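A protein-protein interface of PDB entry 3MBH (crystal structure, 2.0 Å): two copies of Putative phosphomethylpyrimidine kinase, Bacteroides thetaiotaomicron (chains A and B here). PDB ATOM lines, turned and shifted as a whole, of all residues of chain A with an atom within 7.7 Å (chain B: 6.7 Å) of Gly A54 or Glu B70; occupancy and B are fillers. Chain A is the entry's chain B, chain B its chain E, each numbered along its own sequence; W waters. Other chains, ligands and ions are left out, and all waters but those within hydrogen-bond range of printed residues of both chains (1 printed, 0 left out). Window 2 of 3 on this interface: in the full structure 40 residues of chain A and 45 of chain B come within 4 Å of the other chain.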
ATOM      1  N   LEU A  46     -23.628 -21.986 -14.876  1.00  0.00           N
ATOM      2  CA  LEU A  46     -22.518 -21.094 -15.176  1.00  0.00           C
ATOM      3  C   LEU A  46     -23.024 -19.677 -15.579  1.00  0.00           C
ATOM      4  O   LEU A  46     -24.094 -19.552 -16.121  1.00  0.00           O
ATOM      5  CB  LEU A  46     -21.682 -21.660 -16.330  1.00  0.00           C
ATOM      6  CG  LEU A  46     -21.090 -23.048 -16.209  1.00  0.00           C
ATOM      7  CD1 LEU A  46     -22.195 -24.141 -16.557  1.00  0.00           C
ATOM      8  CD2 LEU A  46     -19.877 -23.087 -17.130  1.00  0.00           C
ATOM      9  N   SER A  47     -22.197 -18.665 -15.375  1.00  0.00           N
ATOM     10  CA  SER A  47     -22.381 -17.324 -15.885  1.00  0.00           C
ATOM     11  C   SER A  47     -22.361 -17.259 -17.393  1.00  0.00           C
ATOM     12  O   SER A  47     -23.089 -16.452 -18.024  1.00  0.00           O
ATOM     13  CB  SER A  47     -21.274 -16.406 -15.334  1.00  0.00           C
ATOM     14  OG  SER A  47     -19.966 -16.927 -15.650  1.00  0.00           O
ATOM     15  N   ASN A  48     -21.531 -18.113 -17.975  1.00  0.00           N
ATOM     16  CA  ASN A  48     -21.318 -18.121 -19.416  1.00  0.00           C
ATOM     17  C   ASN A  48     -20.586 -19.391 -19.798  1.00  0.00           C
ATOM     18  O   ASN A  48     -20.099 -20.136 -18.934  1.00  0.00           O
ATOM     19  CB  ASN A  48     -20.505 -16.868 -19.855  1.00  0.00           C
ATOM     20  CG  ASN A  48     -19.308 -16.614 -18.980  1.00  0.00           C
ATOM     21  OD1 ASN A  48     -19.421 -15.898 -17.975  1.00  0.00           O
ATOM     22  ND2 ASN A  48     -18.164 -17.232 -19.304  1.00  0.00           N
ATOM     23  N   HIS A  49     -20.485 -19.660 -21.087  1.00  0.00           N
ATOM     24  CA  HIS A  49     -19.772 -20.840 -21.521  1.00  0.00           C
ATOM     25  C   HIS A  49     -18.284 -20.749 -21.215  1.00  0.00           C
ATOM     26  O   HIS A  49     -17.701 -19.659 -20.885  1.00  0.00           O
ATOM     27  CB  HIS A  49     -20.037 -21.188 -22.998  1.00  0.00           C
ATOM     28  CG  HIS A  49     -19.534 -20.176 -23.956  1.00  0.00           C
ATOM     29  ND1 HIS A  49     -18.206 -19.797 -24.001  1.00  0.00           N
ATOM     30  CD2 HIS A  49     -20.173 -19.460 -24.926  1.00  0.00           C
ATOM     31  CE1 HIS A  49     -18.049 -18.879 -24.956  1.00  0.00           C
ATOM     32  NE2 HIS A  49     -19.233 -18.641 -25.516  1.00  0.00           N
ATOM     33  N   THR A  50     -17.658 -21.916 -21.262  1.00  0.00           N
ATOM     34  CA  THR A  50     -16.259 -22.039 -20.824  1.00  0.00           C
ATOM     35  C   THR A  50     -15.255 -21.781 -21.925  1.00  0.00           C
ATOM     36  O   THR A  50     -14.045 -21.988 -21.705  1.00  0.00           O
ATOM     37  CB  THR A  50     -15.968 -23.369 -20.196  1.00  0.00           C
ATOM     38  OG1 THR A  50     -16.064 -24.404 -21.189  1.00  0.00           O
ATOM     39  CG2 THR A  50     -16.970 -23.626 -19.041  1.00  0.00           C
ATOM     40  N   GLN A  51     -15.700 -21.233 -23.068  1.00  0.00           N
ATOM     41  CA  GLN A  51     -14.709 -20.723 -24.038  1.00  0.00           C
ATOM     42  C   GLN A  51     -14.416 -19.216 -23.896  1.00  0.00           C
ATOM     43  O   GLN A  51     -13.540 -18.678 -24.560  1.00  0.00           O
ATOM     44  CB  GLN A  51     -15.114 -21.114 -25.439  1.00  0.00           C
ATOM     45  CG  GLN A  51     -15.156 -22.642 -25.630  1.00  0.00           C
ATOM     46  CD  GLN A  51     -15.453 -23.000 -27.073  1.00  0.00           C
ATOM     47  OE1 GLN A  51     -14.786 -22.498 -27.959  1.00  0.00           O
ATOM     48  NE2 GLN A  51     -16.485 -23.819 -27.319  1.00  0.00           N
ATOM     49  N   TYR A  52     -15.125 -18.561 -22.983  1.00  0.00           N
ATOM     50  CA  TYR A  52     -14.712 -17.305 -22.436  1.00  0.00           C
ATOM     51  C   TYR A  52     -13.586 -17.626 -21.471  1.00  0.00           C
ATOM     52  O   TYR A  52     -13.505 -18.762 -20.975  1.00  0.00           O
ATOM     53  CB  TYR A  52     -15.878 -16.617 -21.705  1.00  0.00           C
ATOM     54  CG  TYR A  52     -16.867 -15.890 -22.619  1.00  0.00           C
ATOM     55  CD1 TYR A  52     -16.541 -14.684 -23.214  1.00  0.00           C
ATOM     56  CD2 TYR A  52     -18.137 -16.392 -22.832  1.00  0.00           C
ATOM     57  CE1 TYR A  52     -17.467 -14.011 -24.014  1.00  0.00           C
ATOM     58  CE2 TYR A  52     -19.053 -15.744 -23.628  1.00  0.00           C
ATOM     59  CZ  TYR A  52     -18.706 -14.570 -24.242  1.00  0.00           C
ATOM     60  OH  TYR A  52     -19.617 -13.943 -25.044  1.00  0.00           O
ATOM     61  N   PRO A  53     -12.747 -16.627 -21.151  1.00  0.00           N
ATOM     62  CA  PRO A  53     -11.621 -16.913 -20.276  1.00  0.00           C
ATOM     63  C   PRO A  53     -12.013 -17.210 -18.820  1.00  0.00           C
ATOM     64  O   PRO A  53     -11.294 -17.949 -18.131  1.00  0.00           O
ATOM     65  CB  PRO A  53     -10.746 -15.658 -20.393  1.00  0.00           C
ATOM     66  CG  PRO A  53     -11.603 -14.612 -20.971  1.00  0.00           C
ATOM     67  CD  PRO A  53     -12.826 -15.213 -21.524  1.00  0.00           C
ATOM     68  N   GLY A  54     -13.117 -16.652 -18.361  1.00  0.00           N
ATOM     69  CA  GLY A  54     -13.537 -16.808 -16.999  1.00  0.00           C
ATOM     70  C   GLY A  54     -14.992 -17.199 -16.995  1.00  0.00           C
ATOM     71  O   GLY A  54     -15.715 -16.925 -17.956  1.00  0.00           O
ATOM     72  N   PHE A  55     -15.409 -17.852 -15.924  1.00  0.00           N
ATOM     73  CA  PHE A  55     -16.784 -18.255 -15.779  1.00  0.00           C
ATOM     74  C   PHE A  55     -17.030 -18.673 -14.316  1.00  0.00           C
ATOM     75  O   PHE A  55     -16.135 -19.157 -13.682  1.00  0.00           O
ATOM     76  CB  PHE A  55     -17.135 -19.407 -16.749  1.00  0.00           C
ATOM     77  CG  PHE A  55     -16.214 -20.599 -16.657  1.00  0.00           C
ATOM     78  CD1 PHE A  55     -15.095 -20.696 -17.479  1.00  0.00           C
ATOM     79  CD2 PHE A  55     -16.466 -21.616 -15.756  1.00  0.00           C
ATOM     80  CE1 PHE A  55     -14.202 -21.774 -17.379  1.00  0.00           C
ATOM     81  CE2 PHE A  55     -15.574 -22.717 -15.640  1.00  0.00           C
ATOM     82  CZ  PHE A  55     -14.467 -22.789 -16.477  1.00  0.00           C
ATOM     83  N   SER A  56     -18.224 -18.437 -13.787  1.00  0.00           N
ATOM     84  CA  SER A  56     -18.657 -19.040 -12.516  1.00  0.00           C
ATOM     85  C   SER A  56     -19.063 -20.474 -12.853  1.00  0.00           C
ATOM     86  O   SER A  56     -19.438 -20.763 -13.990  1.00  0.00           O
ATOM     87  CB  SER A  56     -19.829 -18.261 -11.880  1.00  0.00           C
ATOM     88  OG  SER A  56     -20.974 -18.239 -12.724  1.00  0.00           O
ATOM     89  N   PHE A  57     -18.990 -21.363 -11.868  1.00  0.00           N
ATOM     90  CA  PHE A  57     -19.381 -22.730 -12.091  1.00  0.00           C
ATOM     91  C   PHE A  57     -19.946 -23.371 -10.851  1.00  0.00           C
ATOM     92  O   PHE A  57     -19.288 -23.429  -9.806  1.00  0.00           O
ATOM     93  CB  PHE A  57     -18.189 -23.538 -12.623  1.00  0.00           C
ATOM     94  CG  PHE A  57     -18.522 -24.967 -12.957  1.00  0.00           C
ATOM     95  CD1 PHE A  57     -18.991 -25.313 -14.200  1.00  0.00           C
ATOM     96  CD2 PHE A  57     -18.321 -25.992 -12.023  1.00  0.00           C
ATOM     97  CE1 PHE A  57     -19.288 -26.635 -14.515  1.00  0.00           C
ATOM     98  CE2 PHE A  57     -18.611 -27.341 -12.339  1.00  0.00           C
ATOM     99  CZ  PHE A  57     -19.125 -27.644 -13.579  1.00  0.00           C
ATOM    100  N   ARG A 267     -17.874 -15.256 -29.752  1.00  0.00           N
ATOM    101  CA  ARG A 267     -18.121 -16.048 -28.543  1.00  0.00           C
ATOM    102  C   ARG A 267     -19.574 -15.955 -28.094  1.00  0.00           C
ATOM    103  O   ARG A 267     -20.067 -16.811 -27.340  1.00  0.00           O
ATOM    104  CB  ARG A 267     -17.154 -15.609 -27.439  1.00  0.00           C
ATOM    105  CG  ARG A 267     -15.654 -15.829 -27.824  1.00  0.00           C
ATOM    106  CD  ARG A 267     -14.696 -15.342 -26.762  1.00  0.00           C
ATOM    107  NE  ARG A 267     -14.855 -13.906 -26.595  1.00  0.00           N
ATOM    108  CZ  ARG A 267     -14.137 -13.161 -25.772  1.00  0.00           C
ATOM    109  NH1 ARG A 267     -13.190 -13.676 -25.003  1.00  0.00           N
ATOM    110  NH2 ARG A 267     -14.395 -11.881 -25.700  1.00  0.00           N
ATOM    111  N   PRO B  65     -24.407 -13.755  -6.877  1.00  0.00           N
ATOM    112  CA  PRO B  65     -23.346 -12.764  -6.941  1.00  0.00           C
ATOM    113  C   PRO B  65     -22.142 -13.230  -7.775  1.00  0.00           C
ATOM    114  O   PRO B  65     -21.466 -12.413  -8.383  1.00  0.00           O
ATOM    115  CB  PRO B  65     -22.955 -12.559  -5.462  1.00  0.00           C
ATOM    116  CG  PRO B  65     -24.130 -13.009  -4.670  1.00  0.00           C
ATOM    117  CD  PRO B  65     -24.723 -14.131  -5.487  1.00  0.00           C
ATOM    118  N   LYS B  66     -21.884 -14.537  -7.820  1.00  0.00           N
ATOM    119  CA  LYS B  66     -20.737 -15.068  -8.564  1.00  0.00           C
ATOM    120  C   LYS B  66     -21.005 -14.895 -10.066  1.00  0.00           C
ATOM    121  O   LYS B  66     -20.095 -14.536 -10.829  1.00  0.00           O
ATOM    122  CB  LYS B  66     -20.456 -16.521  -8.210  1.00  0.00           C
ATOM    123  CG  LYS B  66     -20.145 -16.711  -6.767  1.00  0.00           C
ATOM    124  CD  LYS B  66     -19.907 -18.152  -6.397  1.00  0.00           C
ATOM    125  CE  LYS B  66     -19.603 -18.227  -4.908  1.00  0.00           C
ATOM    126  NZ  LYS B  66     -19.187 -19.566  -4.529  1.00  0.00           N
ATOM    127  N   ILE B  67     -22.261 -15.114 -10.463  1.00  0.00           N
ATOM    128  CA  ILE B  67     -22.660 -14.927 -11.853  1.00  0.00           C
ATOM    129  C   ILE B  67     -22.566 -13.442 -12.257  1.00  0.00           C
ATOM    130  O   ILE B  67     -21.944 -13.093 -13.281  1.00  0.00           O
ATOM    131  CB  ILE B  67     -24.107 -15.434 -12.125  1.00  0.00           C
ATOM    132  CG1 ILE B  67     -24.138 -16.938 -11.950  1.00  0.00           C
ATOM    133  CG2 ILE B  67     -24.543 -15.060 -13.571  1.00  0.00           C
ATOM    134  CD1 ILE B  67     -25.586 -17.590 -11.981  1.00  0.00           C
ATOM    135  N   ILE B  68     -23.177 -12.587 -11.420  1.00  0.00           N
ATOM    136  CA  ILE B  68     -23.184 -11.140 -11.632  1.00  0.00           C
ATOM    137  C   ILE B  68     -21.761 -10.584 -11.759  1.00  0.00           C
ATOM    138  O   ILE B  68     -21.471  -9.791 -12.666  1.00  0.00           O
ATOM    139  CB  ILE B  68     -24.005 -10.393 -10.575  1.00  0.00           C
ATOM    140  CG1 ILE B  68     -25.511 -10.745 -10.724  1.00  0.00           C
ATOM    141  CG2 ILE B  68     -23.722  -8.867 -10.736  1.00  0.00           C
ATOM    142  CD1 ILE B  68     -26.367 -10.497  -9.472  1.00  0.00           C
ATOM    143  N   ALA B  69     -20.867 -10.991 -10.859  1.00  0.00           N
ATOM    144  CA  ALA B  69     -19.457 -10.570 -10.948  1.00  0.00           C
ATOM    145  C   ALA B  69     -18.843 -10.990 -12.304  1.00  0.00           C
ATOM    146  O   ALA B  69     -18.020 -10.268 -12.876  1.00  0.00           O
ATOM    147  CB  ALA B  69     -18.639 -11.193  -9.799  1.00  0.00           C
ATOM    148  N   GLU B  70     -19.198 -12.163 -12.813  1.00  0.00           N
ATOM    149  CA  GLU B  70     -18.630 -12.541 -14.116  1.00  0.00           C
ATOM    150  C   GLU B  70     -19.235 -11.721 -15.222  1.00  0.00           C
ATOM    151  O   GLU B  70     -18.533 -11.308 -16.155  1.00  0.00           O
ATOM    152  CB  GLU B  70     -18.775 -14.024 -14.457  1.00  0.00           C
ATOM    153  CG  GLU B  70     -17.949 -14.975 -13.595  1.00  0.00           C
ATOM    154  CD  GLU B  70     -16.468 -14.720 -13.525  1.00  0.00           C
ATOM    155  OE1 GLU B  70     -15.780 -14.481 -14.549  1.00  0.00           O
ATOM    156  OE2 GLU B  70     -15.955 -14.827 -12.386  1.00  0.00           O
ATOM    157  N   TRP B  71     -20.537 -11.463 -15.134  1.00  0.00           N
ATOM    158  CA  TRP B  71     -21.167 -10.613 -16.136  1.00  0.00           C
ATOM    159  C   TRP B  71     -20.545  -9.188 -16.162  1.00  0.00           C
ATOM    160  O   TRP B  71     -20.384  -8.587 -17.240  1.00  0.00           O
ATOM    161  CB  TRP B  71     -22.654 -10.548 -15.921  1.00  0.00           C
ATOM    162  CG  TRP B  71     -23.414 -11.799 -16.308  1.00  0.00           C
ATOM    163  CD1 TRP B  71     -22.934 -12.878 -16.974  1.00  0.00           C
ATOM    164  CD2 TRP B  71     -24.807 -12.032 -16.133  1.00  0.00           C
ATOM    165  NE1 TRP B  71     -23.911 -13.782 -17.167  1.00  0.00           N
ATOM    166  CE2 TRP B  71     -25.087 -13.289 -16.676  1.00  0.00           C
ATOM    167  CE3 TRP B  71     -25.838 -11.294 -15.581  1.00  0.00           C
ATOM    168  CZ2 TRP B  71     -26.374 -13.828 -16.695  1.00  0.00           C
ATOM    169  CZ3 TRP B  71     -27.100 -11.805 -15.589  1.00  0.00           C
ATOM    170  CH2 TRP B  71     -27.361 -13.072 -16.150  1.00  0.00           C
ATOM    171  N   LYS B  72     -20.153  -8.655 -15.003  1.00  0.00           N
ATOM    172  CA  LYS B  72     -19.502  -7.361 -15.000  1.00  0.00           C
ATOM    173  C   LYS B  72     -18.168  -7.440 -15.726  1.00  0.00           C
ATOM    174  O   LYS B  72     -17.821  -6.558 -16.524  1.00  0.00           O
ATOM    175  CB  LYS B  72     -19.320  -6.831 -13.585  1.00  0.00           C
ATOM    176  CG  LYS B  72     -20.665  -6.452 -12.956  1.00  0.00           C
ATOM    177  CD  LYS B  72     -20.492  -5.754 -11.581  1.00  0.00           C
ATOM    178  CE  LYS B  72     -21.854  -5.507 -10.882  1.00  0.00           C
ATOM    179  NZ  LYS B  72     -21.761  -4.607  -9.686  1.00  0.00           N
ATOM    180  N   LYS B  73     -17.409  -8.492 -15.449  1.00  0.00           N
ATOM    181  CA  LYS B  73     -16.140  -8.712 -16.123  1.00  0.00           C
ATOM    182  C   LYS B  73     -16.284  -8.826 -17.645  1.00  0.00           C
ATOM    183  O   LYS B  73     -15.371  -8.428 -18.383  1.00  0.00           O
ATOM    184  CB  LYS B  73     -15.469  -9.975 -15.593  1.00  0.00           C
ATOM    185  CG  LYS B  73     -14.872  -9.815 -14.229  1.00  0.00           C
ATOM    186  CD  LYS B  73     -14.276 -11.126 -13.755  1.00  0.00           C
ATOM    187  CE  LYS B  73     -13.889 -11.071 -12.276  1.00  0.00           C
ATOM    188  NZ  LYS B  73     -14.342 -12.348 -11.628  1.00  0.00           N
ATOM    189  N   LEU B  74     -17.378  -9.427 -18.103  1.00  0.00           N
ATOM    190  CA  LEU B  74     -17.639  -9.560 -19.533  1.00  0.00           C
ATOM    191  C   LEU B  74     -18.049  -8.260 -20.189  1.00  0.00           C
ATOM    192  O   LEU B  74     -18.076  -8.193 -21.393  1.00  0.00           O
ATOM    193  CB  LEU B  74     -18.759 -10.572 -19.823  1.00  0.00           C
ATOM    194  CG  LEU B  74     -18.431 -12.043 -19.548  1.00  0.00           C
ATOM    195  CD1 LEU B  74     -19.748 -12.892 -19.817  1.00  0.00           C
ATOM    196  CD2 LEU B  74     -17.196 -12.467 -20.358  1.00  0.00           C
ATOM    197  N   GLU B  75     -18.422  -7.265 -19.393  1.00  0.00           N
ATOM    198  CA  GLU B  75     -18.958  -6.005 -19.867  1.00  0.00           C
ATOM    199  C   GLU B  75     -20.276  -6.191 -20.577  1.00  0.00           C
ATOM    200  O   GLU B  75     -20.553  -5.494 -21.518  1.00  0.00           O
ATOM    201  CB  GLU B  75     -17.948  -5.284 -20.770  1.00  0.00           C
ATOM    202  CG  GLU B  75     -16.589  -5.217 -20.174  1.00  0.00           C
ATOM    203  CD  GLU B  75     -15.694  -4.124 -20.747  1.00  0.00           C
ATOM    204  OE1 GLU B  75     -16.161  -3.229 -21.491  1.00  0.00           O
ATOM    205  OE2 GLU B  75     -14.509  -4.171 -20.453  1.00  0.00           O
ATOM    206  N   VAL B  76     -21.118  -7.119 -20.123  1.00  0.00           N
ATOM    207  CA  VAL B  76     -22.365  -7.398 -20.844  1.00  0.00           C
ATOM    208  C   VAL B  76     -23.339  -6.308 -20.508  1.00  0.00           C
ATOM    209  O   VAL B  76     -23.365  -5.844 -19.391  1.00  0.00           O
ATOM    210  CB  VAL B  76     -22.961  -8.803 -20.492  1.00  0.00           C
ATOM    211  CG1 VAL B  76     -22.968  -9.028 -19.026  1.00  0.00           C
ATOM    212  CG2 VAL B  76     -24.400  -8.981 -21.040  1.00  0.00           C
HETATM  213  O   HOH W   1     -19.886 -22.040  -6.866  1.00  0.00           O
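OD1 of Asn A48 sits at hydrogen-bond distance from OG of Ser A47 (2.6 Å). A ring nitrogen (ND1) of His A49 is in hydrogen-bond range of the backbone NH (N) of Tyr A52, 3.5 Å away. The side-chain hydroxyl of Ser A56 is in hydrogen-bond range of the backbone NH of Ser A47, at 3.0 Å. The side-chain carboxylate of Glu B70 is in salt-bridge range of the side-chain amino group of Lys B73 (3.1 Å). The backbone carbonyl oxygen (O) of Gly A54 lies within hydrogen-bond range of the side-chain amide nitrogen (ND2) of Asn A48. The backbone NH (N) of Val B76 sits close to the backbone carbonyl oxygen (O) of Trp B71 (3.3 Å).
Among the printed residues, merely in contact across the chains: Ser A47 with Ile B67 (3.9 Å), Ser A47 with Glu B70 (3.4 Å), Asn A48 with Leu B74 (3.5 Å), Tyr A52 with Leu B74 (3.7 Å), Gly A54 with Glu B70 (3.7 Å), Phe A55 with Glu B70 (3.7 Å), Ser A56 with Lys B66 (3.9 Å), Ser A56 with Ile B67 (3.5 Å) and Ser A56 with Glu B70 (3.5 Å).
Printed residues of chain A that touch a printed residue of chain B: Ser A47, Asn A48, Tyr A52, Gly A54, Phe A55 and Ser A56. Hydrophobic or aromatic side chains of chain A that line the printed part of chain B: Tyr A52. Along chain A the printed residues that touch a printed residue of chain B span positions 47 to 56. Hydrophobic or aromatic side chains of chain B within 4 Å of the printed part of chain A: Ile B67, Trp B71 and Leu B74. Among the printed residues, 10 pairs touch across the chains.
No position is printed for both chains. Of the 10 pairs that touch across the chains among the printed residues, none has its exchanged pair printed and touching as well.
Water W1 lies within hydrogen-bond range of the backbone carbonyl oxygen of Phe A57 and the side-chain amino group of Lys B66.
O of Ser A47 lies within hydrogen-bond range of NE1 of Trp B71 (2.9 Å).
Of the printed residues of chain B, Asn A48 touches Leu B74. Of the printed residues of chain B, Tyr A52 touches Leu B74 (3.7 Å). Of the printed residues of chain B, Ser A56 touches Lys B66 (3.9 Å), Ile B67 (3.5 Å) and Glu B70 (3.5 Å). Of the printed residues of chain A, Ile B67 touches Ser A47 (3.9 Å) and Ser A56 (3.5 Å). No residue of chain A comes within 4 Å of Ala B69. Glu B70 touches just these residues of chain A: Ser A47, Gly A54, Phe A55 and Ser A56. Printed residues of chain A within 4 Å of Trp B71: Ser A47 (2.9 Å). The nearest residue of chain B that does not touch Gly A54 is Leu B74 (5.3 Å).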
